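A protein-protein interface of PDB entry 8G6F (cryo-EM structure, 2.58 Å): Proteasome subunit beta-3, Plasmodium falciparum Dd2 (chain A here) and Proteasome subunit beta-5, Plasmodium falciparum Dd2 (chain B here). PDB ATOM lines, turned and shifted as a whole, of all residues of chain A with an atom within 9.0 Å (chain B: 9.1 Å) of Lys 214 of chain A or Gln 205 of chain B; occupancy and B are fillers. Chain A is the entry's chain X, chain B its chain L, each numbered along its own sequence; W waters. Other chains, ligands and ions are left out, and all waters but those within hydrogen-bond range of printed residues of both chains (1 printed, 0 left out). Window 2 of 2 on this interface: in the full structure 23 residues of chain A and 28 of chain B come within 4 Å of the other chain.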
ATOM      1  N   LEU A  27       3.382 -19.854 -22.836  1.00  0.00           N
ATOM      2  CA  LEU A  27       3.548 -20.226 -21.435  1.00  0.00           C
ATOM      3  C   LEU A  27       4.111 -21.629 -21.232  1.00  0.00           C
ATOM      4  O   LEU A  27       4.141 -22.110 -20.098  1.00  0.00           O
ATOM      5  CB  LEU A  27       2.211 -20.104 -20.702  1.00  0.00           C
ATOM      6  CG  LEU A  27       1.726 -18.684 -20.422  1.00  0.00           C
ATOM      7  CD1 LEU A  27       0.291 -18.705 -19.958  1.00  0.00           C
ATOM      8  CD2 LEU A  27       2.609 -18.006 -19.394  1.00  0.00           C
ATOM      9  N   PHE A 177      -4.615  -5.148 -28.451  1.00  0.00           N
ATOM     10  CA  PHE A 177      -4.716  -6.444 -27.795  1.00  0.00           C
ATOM     11  C   PHE A 177      -5.285  -7.489 -28.741  1.00  0.00           C
ATOM     12  O   PHE A 177      -4.772  -8.609 -28.827  1.00  0.00           O
ATOM     13  CB  PHE A 177      -5.584  -6.342 -26.543  1.00  0.00           C
ATOM     14  CG  PHE A 177      -6.139  -7.657 -26.099  1.00  0.00           C
ATOM     15  CD1 PHE A 177      -5.352  -8.551 -25.400  1.00  0.00           C
ATOM     16  CD2 PHE A 177      -7.437  -8.013 -26.404  1.00  0.00           C
ATOM     17  CE1 PHE A 177      -5.850  -9.765 -25.008  1.00  0.00           C
ATOM     18  CE2 PHE A 177      -7.940  -9.228 -26.012  1.00  0.00           C
ATOM     19  CZ  PHE A 177      -7.148 -10.105 -25.313  1.00  0.00           C
ATOM     20  N   SER A 181      -3.020 -10.667 -29.886  1.00  0.00           N
ATOM     21  CA  SER A 181      -3.503 -11.983 -29.493  1.00  0.00           C
ATOM     22  C   SER A 181      -3.742 -12.861 -30.709  1.00  0.00           C
ATOM     23  O   SER A 181      -3.379 -14.041 -30.709  1.00  0.00           O
ATOM     24  CB  SER A 181      -4.786 -11.851 -28.680  1.00  0.00           C
ATOM     25  OG  SER A 181      -4.688 -10.804 -27.738  1.00  0.00           O
ATOM     26  N   GLN A 182      -4.354 -12.309 -31.756  1.00  0.00           N
ATOM     27  CA  GLN A 182      -4.603 -13.107 -32.948  1.00  0.00           C
ATOM     28  C   GLN A 182      -3.301 -13.531 -33.606  1.00  0.00           C
ATOM     29  O   GLN A 182      -3.148 -14.692 -34.004  1.00  0.00           O
ATOM     30  CB  GLN A 182      -5.473 -12.323 -33.927  1.00  0.00           C
ATOM     31  CG  GLN A 182      -6.932 -12.241 -33.521  1.00  0.00           C
ATOM     32  CD  GLN A 182      -7.532 -13.597 -33.251  1.00  0.00           C
ATOM     33  OE1 GLN A 182      -7.332 -14.535 -34.015  1.00  0.00           O
ATOM     34  NE2 GLN A 182      -8.266 -13.712 -32.158  1.00  0.00           N
ATOM     35  N   LEU A 185      -1.723 -16.310 -31.397  1.00  0.00           N
ATOM     36  CA  LEU A 185      -2.448 -17.574 -31.410  1.00  0.00           C
ATOM     37  C   LEU A 185      -2.300 -18.283 -32.747  1.00  0.00           C
ATOM     38  O   LEU A 185      -2.069 -19.497 -32.790  1.00  0.00           O
ATOM     39  CB  LEU A 185      -3.920 -17.334 -31.085  1.00  0.00           C
ATOM     40  CG  LEU A 185      -4.217 -16.974 -29.629  1.00  0.00           C
ATOM     41  CD1 LEU A 185      -5.653 -16.517 -29.471  1.00  0.00           C
ATOM     42  CD2 LEU A 185      -3.932 -18.147 -28.717  1.00  0.00           C
ATOM     43  N   ASP A 189      -0.409 -21.886 -33.263  1.00  0.00           N
ATOM     44  CA  ASP A 189      -1.146 -23.051 -33.729  1.00  0.00           C
ATOM     45  C   ASP A 189      -0.351 -23.879 -34.727  1.00  0.00           C
ATOM     46  O   ASP A 189      -0.713 -25.030 -34.984  1.00  0.00           O
ATOM     47  CB  ASP A 189      -2.467 -22.612 -34.354  1.00  0.00           C
ATOM     48  CG  ASP A 189      -3.488 -22.195 -33.319  1.00  0.00           C
ATOM     49  OD1 ASP A 189      -3.133 -22.122 -32.126  1.00  0.00           O
ATOM     50  OD2 ASP A 189      -4.650 -21.941 -33.697  1.00  0.00           O
ATOM     51  N   TRP A 196       0.573 -24.031 -25.399  1.00  0.00           N
ATOM     52  CA  TRP A 196       0.091 -24.417 -24.076  1.00  0.00           C
ATOM     53  C   TRP A 196      -0.214 -23.187 -23.225  1.00  0.00           C
ATOM     54  O   TRP A 196       0.135 -23.115 -22.045  1.00  0.00           O
ATOM     55  CB  TRP A 196       1.096 -25.325 -23.373  1.00  0.00           C
ATOM     56  CG  TRP A 196       1.077 -26.736 -23.856  1.00  0.00           C
ATOM     57  CD1 TRP A 196       0.345 -27.763 -23.350  1.00  0.00           C
ATOM     58  CD2 TRP A 196       1.836 -27.279 -24.940  1.00  0.00           C
ATOM     59  NE1 TRP A 196       0.599 -28.913 -24.048  1.00  0.00           N
ATOM     60  CE2 TRP A 196       1.509 -28.641 -25.034  1.00  0.00           C
ATOM     61  CE3 TRP A 196       2.757 -26.745 -25.842  1.00  0.00           C
ATOM     62  CZ2 TRP A 196       2.073 -29.476 -25.988  1.00  0.00           C
ATOM     63  CZ3 TRP A 196       3.311 -27.569 -26.787  1.00  0.00           C
ATOM     64  CH2 TRP A 196       2.972 -28.920 -26.854  1.00  0.00           C
ATOM     65  N   GLY A 197      -0.871 -22.215 -23.827  1.00  0.00           N
ATOM     66  CA  GLY A 197      -1.254 -21.010 -23.126  1.00  0.00           C
ATOM     67  C   GLY A 197      -0.466 -19.807 -23.606  1.00  0.00           C
ATOM     68  O   GLY A 197       0.710 -19.901 -23.975  1.00  0.00           O
ATOM     69  N   ALA A 198      -1.122 -18.652 -23.583  1.00  0.00           N
ATOM     70  CA  ALA A 198      -0.522 -17.405 -24.033  1.00  0.00           C
ATOM     71  C   ALA A 198      -0.818 -16.312 -23.022  1.00  0.00           C
ATOM     72  O   ALA A 198      -1.952 -16.185 -22.555  1.00  0.00           O
ATOM     73  CB  ALA A 198      -1.054 -17.005 -25.408  1.00  0.00           C
ATOM     74  N   GLU A 199       0.203 -15.531 -22.687  1.00  0.00           N
ATOM     75  CA  GLU A 199       0.081 -14.411 -21.765  1.00  0.00           C
ATOM     76  C   GLU A 199       0.309 -13.121 -22.538  1.00  0.00           C
ATOM     77  O   GLU A 199       1.297 -13.001 -23.264  1.00  0.00           O
ATOM     78  CB  GLU A 199       1.090 -14.541 -20.624  1.00  0.00           C
ATOM     79  CG  GLU A 199       1.222 -13.318 -19.739  1.00  0.00           C
ATOM     80  CD  GLU A 199       2.164 -13.550 -18.574  1.00  0.00           C
ATOM     81  OE1 GLU A 199       1.804 -14.323 -17.662  1.00  0.00           O
ATOM     82  OE2 GLU A 199       3.264 -12.960 -18.562  1.00  0.00           O
ATOM     83  N   VAL A 200      -0.607 -12.166 -22.389  1.00  0.00           N
ATOM     84  CA  VAL A 200      -0.550 -10.899 -23.111  1.00  0.00           C
ATOM     85  C   VAL A 200      -0.645  -9.762 -22.105  1.00  0.00           C
ATOM     86  O   VAL A 200      -1.595  -9.704 -21.318  1.00  0.00           O
ATOM     87  CB  VAL A 200      -1.668 -10.782 -24.158  1.00  0.00           C
ATOM     88  CG1 VAL A 200      -1.516  -9.502 -24.961  1.00  0.00           C
ATOM     89  CG2 VAL A 200      -1.657 -11.982 -25.073  1.00  0.00           C
ATOM     90  N   LYS A 211      -3.651 -10.414 -19.337  1.00  0.00           N
ATOM     91  CA  LYS A 211      -4.673 -11.353 -19.761  1.00  0.00           C
ATOM     92  C   LYS A 211      -4.044 -12.688 -20.117  1.00  0.00           C
ATOM     93  O   LYS A 211      -2.961 -12.743 -20.704  1.00  0.00           O
ATOM     94  CB  LYS A 211      -5.454 -10.816 -20.958  1.00  0.00           C
ATOM     95  CG  LYS A 211      -6.419  -9.708 -20.603  1.00  0.00           C
ATOM     96  CD  LYS A 211      -7.357  -9.417 -21.746  1.00  0.00           C
ATOM     97  CE  LYS A 211      -7.932  -8.023 -21.657  1.00  0.00           C
ATOM     98  NZ  LYS A 211      -8.849  -7.736 -22.782  1.00  0.00           N
ATOM     99  N   LYS A 212      -4.733 -13.761 -19.749  1.00  0.00           N
ATOM    100  CA  LYS A 212      -4.398 -15.106 -20.184  1.00  0.00           C
ATOM    101  C   LYS A 212      -5.401 -15.520 -21.245  1.00  0.00           C
ATOM    102  O   LYS A 212      -6.610 -15.397 -21.041  1.00  0.00           O
ATOM    103  CB  LYS A 212      -4.425 -16.085 -19.013  1.00  0.00           C
ATOM    104  CG  LYS A 212      -3.402 -15.795 -17.948  1.00  0.00           C
ATOM    105  CD  LYS A 212      -2.055 -16.382 -18.302  1.00  0.00           C
ATOM    106  CE  LYS A 212      -0.964 -15.848 -17.394  1.00  0.00           C
ATOM    107  NZ  LYS A 212      -1.409 -15.758 -15.982  1.00  0.00           N
ATOM    108  N   LEU A 213      -4.898 -15.991 -22.379  1.00  0.00           N
ATOM    109  CA  LEU A 213      -5.741 -16.336 -23.510  1.00  0.00           C
ATOM    110  C   LEU A 213      -6.176 -17.788 -23.426  1.00  0.00           C
ATOM    111  O   LEU A 213      -5.409 -18.658 -23.006  1.00  0.00           O
ATOM    112  CB  LEU A 213      -5.001 -16.100 -24.824  1.00  0.00           C
ATOM    113  CG  LEU A 213      -4.433 -14.700 -25.049  1.00  0.00           C
ATOM    114  CD1 LEU A 213      -3.818 -14.618 -26.426  1.00  0.00           C
ATOM    115  CD2 LEU A 213      -5.505 -13.639 -24.868  1.00  0.00           C
ATOM    116  N   LYS A 214      -7.414 -18.045 -23.829  1.00  0.00           N
ATOM    117  CA  LYS A 214      -7.896 -19.409 -23.995  1.00  0.00           C
ATOM    118  C   LYS A 214      -7.278 -19.971 -25.268  1.00  0.00           C
ATOM    119  O   LYS A 214      -7.749 -19.704 -26.374  1.00  0.00           O
ATOM    120  CB  LYS A 214      -9.417 -19.431 -24.056  1.00  0.00           C
ATOM    121  CG  LYS A 214     -10.010 -20.791 -23.802  1.00  0.00           C
ATOM    122  CD  LYS A 214     -11.519 -20.754 -23.794  1.00  0.00           C
ATOM    123  CE  LYS A 214     -12.095 -22.145 -23.955  1.00  0.00           C
ATOM    124  NZ  LYS A 214     -13.577 -22.130 -24.028  1.00  0.00           N
ATOM    125  N   ALA A 215      -6.211 -20.742 -25.117  1.00  0.00           N
ATOM    126  CA  ALA A 215      -5.406 -21.216 -26.231  1.00  0.00           C
ATOM    127  C   ALA A 215      -5.489 -22.735 -26.329  1.00  0.00           C
ATOM    128  O   ALA A 215      -6.103 -23.405 -25.498  1.00  0.00           O
ATOM    129  CB  ALA A 215      -3.952 -20.766 -26.072  1.00  0.00           C
ATOM    130  N   ARG A 216      -4.871 -23.271 -27.375  1.00  0.00           N
ATOM    131  CA  ARG A 216      -4.760 -24.711 -27.537  1.00  0.00           C
ATOM    132  C   ARG A 216      -3.712 -25.272 -26.586  1.00  0.00           C
ATOM    133  O   ARG A 216      -2.709 -24.624 -26.280  1.00  0.00           O
ATOM    134  CB  ARG A 216      -4.388 -25.066 -28.973  1.00  0.00           C
ATOM    135  CG  ARG A 216      -5.406 -24.636 -30.000  1.00  0.00           C
ATOM    136  CD  ARG A 216      -5.042 -25.163 -31.374  1.00  0.00           C
ATOM    137  NE  ARG A 216      -5.239 -26.603 -31.471  1.00  0.00           N
ATOM    138  CZ  ARG A 216      -6.419 -27.191 -31.606  1.00  0.00           C
ATOM    139  NH1 ARG A 216      -7.537 -26.490 -31.679  1.00  0.00           N
ATOM    140  NH2 ARG A 216      -6.477 -28.517 -31.665  1.00  0.00           N
ATOM    141  N   MET A 217      -3.951 -26.495 -26.125  1.00  0.00           N
ATOM    142  CA  MET A 217      -3.065 -27.166 -25.187  1.00  0.00           C
ATOM    143  C   MET A 217      -2.668 -28.534 -25.715  1.00  0.00           C
ATOM    144  O   MET A 217      -2.617 -29.514 -24.970  1.00  0.00           O
ATOM    145  CB  MET A 217      -3.719 -27.290 -23.814  1.00  0.00           C
ATOM    146  CG  MET A 217      -4.386 -26.018 -23.312  1.00  0.00           C
ATOM    147  SD  MET A 217      -3.245 -24.796 -22.650  1.00  0.00           S
ATOM    148  CE  MET A 217      -2.565 -25.664 -21.248  1.00  0.00           C
ATOM    149  N   PHE B 194      -9.184 -29.196 -28.405  1.00  0.00           N
ATOM    150  CA  PHE B 194      -9.363 -27.926 -27.715  1.00  0.00           C
ATOM    151  C   PHE B 194     -10.535 -28.002 -26.744  1.00  0.00           C
ATOM    152  O   PHE B 194     -10.430 -27.575 -25.590  1.00  0.00           O
ATOM    153  CB  PHE B 194      -9.572 -26.812 -28.741  1.00  0.00           C
ATOM    154  CG  PHE B 194      -9.746 -25.450 -28.141  1.00  0.00           C
ATOM    155  CD1 PHE B 194      -8.652 -24.716 -27.733  1.00  0.00           C
ATOM    156  CD2 PHE B 194     -11.003 -24.900 -27.998  1.00  0.00           C
ATOM    157  CE1 PHE B 194      -8.809 -23.462 -27.184  1.00  0.00           C
ATOM    158  CE2 PHE B 194     -11.165 -23.647 -27.452  1.00  0.00           C
ATOM    159  CZ  PHE B 194     -10.066 -22.927 -27.046  1.00  0.00           C
ATOM    160  N   ASP B 195     -11.659 -28.559 -27.194  1.00  0.00           N
ATOM    161  CA  ASP B 195     -12.802 -28.740 -26.307  1.00  0.00           C
ATOM    162  C   ASP B 195     -12.524 -29.790 -25.243  1.00  0.00           C
ATOM    163  O   ASP B 195     -13.024 -29.682 -24.117  1.00  0.00           O
ATOM    164  CB  ASP B 195     -14.032 -29.134 -27.120  1.00  0.00           C
ATOM    165  CG  ASP B 195     -14.243 -28.241 -28.320  1.00  0.00           C
ATOM    166  OD1 ASP B 195     -13.702 -27.118 -28.328  1.00  0.00           O
ATOM    167  OD2 ASP B 195     -14.947 -28.668 -29.260  1.00  0.00           O
ATOM    168  N   LEU B 196     -11.738 -30.814 -25.579  1.00  0.00           N
ATOM    169  CA  LEU B 196     -11.445 -31.862 -24.610  1.00  0.00           C
ATOM    170  C   LEU B 196     -10.655 -31.317 -23.431  1.00  0.00           C
ATOM    171  O   LEU B 196     -10.875 -31.727 -22.289  1.00  0.00           O
ATOM    172  CB  LEU B 196     -10.684 -33.004 -25.281  1.00  0.00           C
ATOM    173  CG  LEU B 196     -11.450 -33.819 -26.323  1.00  0.00           C
ATOM    174  CD1 LEU B 196     -10.653 -35.041 -26.710  1.00  0.00           C
ATOM    175  CD2 LEU B 196     -12.820 -34.220 -25.815  1.00  0.00           C
ATOM    176  N   HIS B 197      -9.717 -30.402 -23.684  1.00  0.00           N
ATOM    177  CA  HIS B 197      -8.938 -29.856 -22.577  1.00  0.00           C
ATOM    178  C   HIS B 197      -9.830 -29.119 -21.587  1.00  0.00           C
ATOM    179  O   HIS B 197      -9.715 -29.302 -20.371  1.00  0.00           O
ATOM    180  CB  HIS B 197      -7.842 -28.922 -23.082  1.00  0.00           C
ATOM    181  CG  HIS B 197      -7.155 -28.174 -21.983  1.00  0.00           C
ATOM    182  ND1 HIS B 197      -6.118 -28.711 -21.253  1.00  0.00           N
ATOM    183  CD2 HIS B 197      -7.376 -26.943 -21.467  1.00  0.00           C
ATOM    184  CE1 HIS B 197      -5.721 -27.839 -20.345  1.00  0.00           C
ATOM    185  NE2 HIS B 197      -6.469 -26.758 -20.455  1.00  0.00           N
ATOM    186  N   TYR B 198     -10.732 -28.284 -22.090  1.00  0.00           N
ATOM    187  CA  TYR B 198     -11.594 -27.494 -21.223  1.00  0.00           C
ATOM    188  C   TYR B 198     -12.815 -28.265 -20.758  1.00  0.00           C
ATOM    189  O   TYR B 198     -13.635 -27.711 -20.024  1.00  0.00           O
ATOM    190  CB  TYR B 198     -12.010 -26.210 -21.938  1.00  0.00           C
ATOM    191  CG  TYR B 198     -10.836 -25.296 -22.175  1.00  0.00           C
ATOM    192  CD1 TYR B 198     -10.311 -24.534 -21.145  1.00  0.00           C
ATOM    193  CD2 TYR B 198     -10.227 -25.224 -23.417  1.00  0.00           C
ATOM    194  CE1 TYR B 198      -9.231 -23.714 -21.349  1.00  0.00           C
ATOM    195  CE2 TYR B 198      -9.144 -24.406 -23.628  1.00  0.00           C
ATOM    196  CZ  TYR B 198      -8.650 -23.654 -22.591  1.00  0.00           C
ATOM    197  OH  TYR B 198      -7.571 -22.834 -22.798  1.00  0.00           O
ATOM    198  N   HIS B 199     -12.969 -29.510 -21.195  1.00  0.00           N
ATOM    199  CA  HIS B 199     -13.937 -30.412 -20.590  1.00  0.00           C
ATOM    200  C   HIS B 199     -13.318 -31.249 -19.477  1.00  0.00           C
ATOM    201  O   HIS B 199     -13.958 -31.482 -18.448  1.00  0.00           O
ATOM    202  CB  HIS B 199     -14.530 -31.324 -21.662  1.00  0.00           C
ATOM    203  CG  HIS B 199     -15.258 -32.508 -21.115  1.00  0.00           C
ATOM    204  ND1 HIS B 199     -16.364 -32.390 -20.301  1.00  0.00           N
ATOM    205  CD2 HIS B 199     -15.045 -33.836 -21.270  1.00  0.00           C
ATOM    206  CE1 HIS B 199     -16.798 -33.594 -19.977  1.00  0.00           C
ATOM    207  NE2 HIS B 199     -16.015 -34.489 -20.552  1.00  0.00           N
ATOM    208  N   TYR B 200     -12.074 -31.690 -19.655  1.00  0.00           N
ATOM    209  CA  TYR B 200     -11.428 -32.602 -18.718  1.00  0.00           C
ATOM    210  C   TYR B 200     -10.662 -31.862 -17.625  1.00  0.00           C
ATOM    211  O   TYR B 200     -10.905 -32.073 -16.434  1.00  0.00           O
ATOM    212  CB  TYR B 200     -10.470 -33.535 -19.470  1.00  0.00           C
ATOM    213  CG  TYR B 200     -11.132 -34.667 -20.219  1.00  0.00           C
ATOM    214  CD1 TYR B 200     -11.980 -35.551 -19.574  1.00  0.00           C
ATOM    215  CD2 TYR B 200     -10.893 -34.859 -21.571  1.00  0.00           C
ATOM    216  CE1 TYR B 200     -12.578 -36.584 -20.256  1.00  0.00           C
ATOM    217  CE2 TYR B 200     -11.485 -35.891 -22.261  1.00  0.00           C
ATOM    218  CZ  TYR B 200     -12.327 -36.751 -21.599  1.00  0.00           C
ATOM    219  OH  TYR B 200     -12.923 -37.785 -22.278  1.00  0.00           O
ATOM    220  N   THR B 201      -9.728 -31.001 -18.018  1.00  0.00           N
ATOM    221  CA  THR B 201      -8.732 -30.462 -17.102  1.00  0.00           C
ATOM    222  C   THR B 201      -9.072 -29.075 -16.577  1.00  0.00           C
ATOM    223  O   THR B 201      -8.808 -28.786 -15.407  1.00  0.00           O
ATOM    224  CB  THR B 201      -7.369 -30.422 -17.793  1.00  0.00           C
ATOM    225  OG1 THR B 201      -7.020 -31.736 -18.239  1.00  0.00           O
ATOM    226  CG2 THR B 201      -6.311 -29.926 -16.853  1.00  0.00           C
ATOM    227  N   ASN B 202      -9.654 -28.207 -17.401  1.00  0.00           N
ATOM    228  CA  ASN B 202      -9.965 -26.831 -17.010  1.00  0.00           C
ATOM    229  C   ASN B 202     -11.421 -26.519 -17.332  1.00  0.00           C
ATOM    230  O   ASN B 202     -11.719 -25.636 -18.140  1.00  0.00           O
ATOM    231  CB  ASN B 202      -9.024 -25.852 -17.709  1.00  0.00           C
ATOM    232  CG  ASN B 202      -8.861 -24.549 -16.948  1.00  0.00           C
ATOM    233  OD1 ASN B 202      -9.368 -24.395 -15.841  1.00  0.00           O
ATOM    234  ND2 ASN B 202      -8.150 -23.602 -17.544  1.00  0.00           N
ATOM    235  N   PRO B 203     -12.360 -27.227 -16.704  1.00  0.00           N
ATOM    236  CA  PRO B 203     -13.780 -26.921 -16.937  1.00  0.00           C
ATOM    237  C   PRO B 203     -14.180 -25.511 -16.541  1.00  0.00           C
ATOM    238  O   PRO B 203     -15.063 -24.928 -17.179  1.00  0.00           O
ATOM    239  CB  PRO B 203     -14.506 -27.974 -16.088  1.00  0.00           C
ATOM    240  CG  PRO B 203     -13.501 -28.439 -15.098  1.00  0.00           C
ATOM    241  CD  PRO B 203     -12.184 -28.358 -15.781  1.00  0.00           C
ATOM    242  N   GLU B 204     -13.564 -24.944 -15.504  1.00  0.00           N
ATOM    243  CA  GLU B 204     -13.993 -23.638 -15.017  1.00  0.00           C
ATOM    244  C   GLU B 204     -13.595 -22.516 -15.965  1.00  0.00           C
ATOM    245  O   GLU B 204     -14.331 -21.533 -16.096  1.00  0.00           O
ATOM    246  CB  GLU B 204     -13.413 -23.382 -13.626  1.00  0.00           C
ATOM    247  CG  GLU B 204     -14.007 -24.237 -12.512  1.00  0.00           C
ATOM    248  CD  GLU B 204     -15.444 -24.655 -12.774  1.00  0.00           C
ATOM    249  OE1 GLU B 204     -16.305 -23.762 -12.922  1.00  0.00           O
ATOM    250  OE2 GLU B 204     -15.713 -25.873 -12.829  1.00  0.00           O
ATOM    251  N   GLN B 205     -12.442 -22.632 -16.619  1.00  0.00           N
ATOM    252  CA  GLN B 205     -11.983 -21.628 -17.576  1.00  0.00           C
ATOM    253  C   GLN B 205     -11.871 -20.248 -16.939  1.00  0.00           C
ATOM    254  O   GLN B 205     -12.096 -19.230 -17.594  1.00  0.00           O
ATOM    255  CB  GLN B 205     -12.903 -21.573 -18.797  1.00  0.00           C
ATOM    256  CG  GLN B 205     -12.732 -22.737 -19.741  1.00  0.00           C
ATOM    257  CD  GLN B 205     -14.009 -23.089 -20.460  1.00  0.00           C
ATOM    258  OE1 GLN B 205     -14.221 -22.688 -21.601  1.00  0.00           O
ATOM    259  NE2 GLN B 205     -14.868 -23.847 -19.798  1.00  0.00           N
ATOM    260  N   LYS B 206     -11.517 -20.201 -15.656  1.00  0.00           N
ATOM    261  CA  LYS B 206     -11.348 -18.946 -14.944  1.00  0.00           C
ATOM    262  C   LYS B 206      -9.890 -18.584 -14.704  1.00  0.00           C
ATOM    263  O   LYS B 206      -9.619 -17.495 -14.188  1.00  0.00           O
ATOM    264  CB  LYS B 206     -12.090 -18.998 -13.602  1.00  0.00           C
ATOM    265  CG  LYS B 206     -11.554 -20.042 -12.633  1.00  0.00           C
ATOM    266  CD  LYS B 206     -12.189 -19.967 -11.246  1.00  0.00           C
ATOM    267  CE  LYS B 206     -13.648 -19.520 -11.257  1.00  0.00           C
ATOM    268  NZ  LYS B 206     -14.540 -20.492 -11.943  1.00  0.00           N
ATOM    269  N   ASP B 207      -8.952 -19.455 -15.058  1.00  0.00           N
ATOM    270  CA  ASP B 207      -7.534 -19.141 -14.955  1.00  0.00           C
ATOM    271  C   ASP B 207      -6.768 -20.115 -15.834  1.00  0.00           C
ATOM    272  O   ASP B 207      -7.311 -21.112 -16.312  1.00  0.00           O
ATOM    273  CB  ASP B 207      -7.045 -19.205 -13.506  1.00  0.00           C
ATOM    274  CG  ASP B 207      -6.061 -18.098 -13.173  1.00  0.00           C
ATOM    275  OD1 ASP B 207      -5.276 -17.704 -14.063  1.00  0.00           O
ATOM    276  OD2 ASP B 207      -6.070 -17.619 -12.020  1.00  0.00           O
ATOM    277  N   GLN B 208      -5.496 -19.804 -16.054  1.00  0.00           N
ATOM    278  CA  GLN B 208      -4.631 -20.694 -16.810  1.00  0.00           C
ATOM    279  C   GLN B 208      -4.335 -21.941 -15.988  1.00  0.00           C
ATOM    280  O   GLN B 208      -3.915 -21.848 -14.831  1.00  0.00           O
ATOM    281  CB  GLN B 208      -3.340 -19.966 -17.186  1.00  0.00           C
ATOM    282  CG  GLN B 208      -2.189 -20.851 -17.643  1.00  0.00           C
ATOM    283  CD  GLN B 208      -2.396 -21.413 -19.028  1.00  0.00           C
ATOM    284  OE1 GLN B 208      -3.395 -21.131 -19.682  1.00  0.00           O
ATOM    285  NE2 GLN B 208      -1.447 -22.214 -19.485  1.00  0.00           N
ATOM    286  N   TYR B 209      -4.553 -23.108 -16.582  1.00  0.00           N
ATOM    287  CA  TYR B 209      -4.291 -24.358 -15.885  1.00  0.00           C
ATOM    288  C   TYR B 209      -2.799 -24.526 -15.642  1.00  0.00           C
ATOM    289  O   TYR B 209      -1.976 -24.249 -16.517  1.00  0.00           O
ATOM    290  CB  TYR B 209      -4.825 -25.537 -16.691  1.00  0.00           C
ATOM    291  CG  TYR B 209      -4.433 -26.877 -16.123  1.00  0.00           C
ATOM    292  CD1 TYR B 209      -5.043 -27.375 -14.984  1.00  0.00           C
ATOM    293  CD2 TYR B 209      -3.443 -27.638 -16.722  1.00  0.00           C
ATOM    294  CE1 TYR B 209      -4.681 -28.594 -14.463  1.00  0.00           C
ATOM    295  CE2 TYR B 209      -3.076 -28.857 -16.208  1.00  0.00           C
ATOM    296  CZ  TYR B 209      -3.696 -29.331 -15.079  1.00  0.00           C
ATOM    297  OH  TYR B 209      -3.330 -30.551 -14.566  1.00  0.00           O
HETATM  298  O   HOH W   1      -3.372 -19.157 -21.340  1.00  0.00           O
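Water W1 lies within hydrogen-bond range of OE1 of Gln 208 of chain B (2.6 Å), O of Leu 213 of chain A (2.7 Å) and N of Ala 198 of chain A (3.2 Å).
Of the 18 printed residues of chain A, 8 touch a printed residue of chain B.
Hydrophobic or aromatic side chains of chain B within 4 Å of the printed part of chain A: Phe 194, His 197 and Tyr 198.
Among the printed residues, no Asp or Glu carboxylate lies within 4 Å of a Lys or Arg side-chain nitrogen of the other chain.
Of the printed residues of chain B, Trp 196 of chain A touches Gln 208 (3.1 Å).
Of the printed residues of chain B, Gly 197 of chain A touches Gln 208.
Val 200 of chain A touches none of the printed residues of chain B.
Lys 214 of chain A touches just these residues of chain B: Phe 194 (3.8 Å), Tyr 198 (3.3 Å) and Gln 205 (2.6 Å).
Ala 215 of chain A touches just these residues of chain B: Phe 194 (3.2 Å) and Tyr 198 (3.1 Å).
Of the printed residues of chain A, Phe 194 of chain B touches Lys 214, Ala 215 and Arg 216.
Of the printed residues of chain A, His 197 of chain B touches Met 217.
Of the printed residues of chain A, Tyr 198 of chain B touches Lys 214 and Ala 215.
Gln 205 of chain B touches just one residue of chain A: Lys 214 (2.6 Å).
Asp 207 of chain B touches none of the printed residues of chain A.
The nearest printed residue of chain A that does not touch Phe 194 of chain B is Met 217 of chain A (5.3 Å).
Among the printed residues, pairs that only touch across the chains: Ala 215 of chain A with Phe 194 of chain B, Lys 214 of chain A with Tyr 198 of chain B, Arg 216 of chain A with Phe 194 of chain B, Met 217 of chain A with His 197 of chain B, Lys 214 of chain A with Phe 194 of chain B, Gly 197 of chain A with Gln 208 of chain B, Leu 27 of chain A with Gln 208 of chain B and Lys 212 of chain A with Gln 208 of chain B.
O of Ala 215 of chain A sits at hydrogen-bond distance from OH of Tyr 198 of chain B (3.1 Å).
O of Trp 196 of chain A is in hydrogen-bond range of NE2 of Gln 208 of chain B (3.1 Å).
The side-chain amide oxygen of Gln 205 of chain B lies within hydrogen-bond range of the side-chain amino group of Lys 214 of chain A, at 2.6 Å.
The side-chain carboxylate (OE1) of Glu 199 of chain A lies within salt-bridge range of the side-chain amino group (NZ) of Lys 212 of chain A, at 3.9 Å.
N of Asn 202 of chain B lies within hydrogen-bond range of O of His 197 of chain B (3.2 Å).
O of Arg 216 of chain A is in hydrogen-bond range of N of Trp 196 of chain A (3.4 Å).
O of Pro 203 of chain B sits at hydrogen-bond distance from NE2 of Gln 205 of chain B (2.8 Å).
SD of Met 217 of chain A is in hydrogen-bond range of N of Gly 197 of chain A.
NE1 of Trp 196 of chain A lies within hydrogen-bond range of O of Met 217 of chain A, at 3.4 Å.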
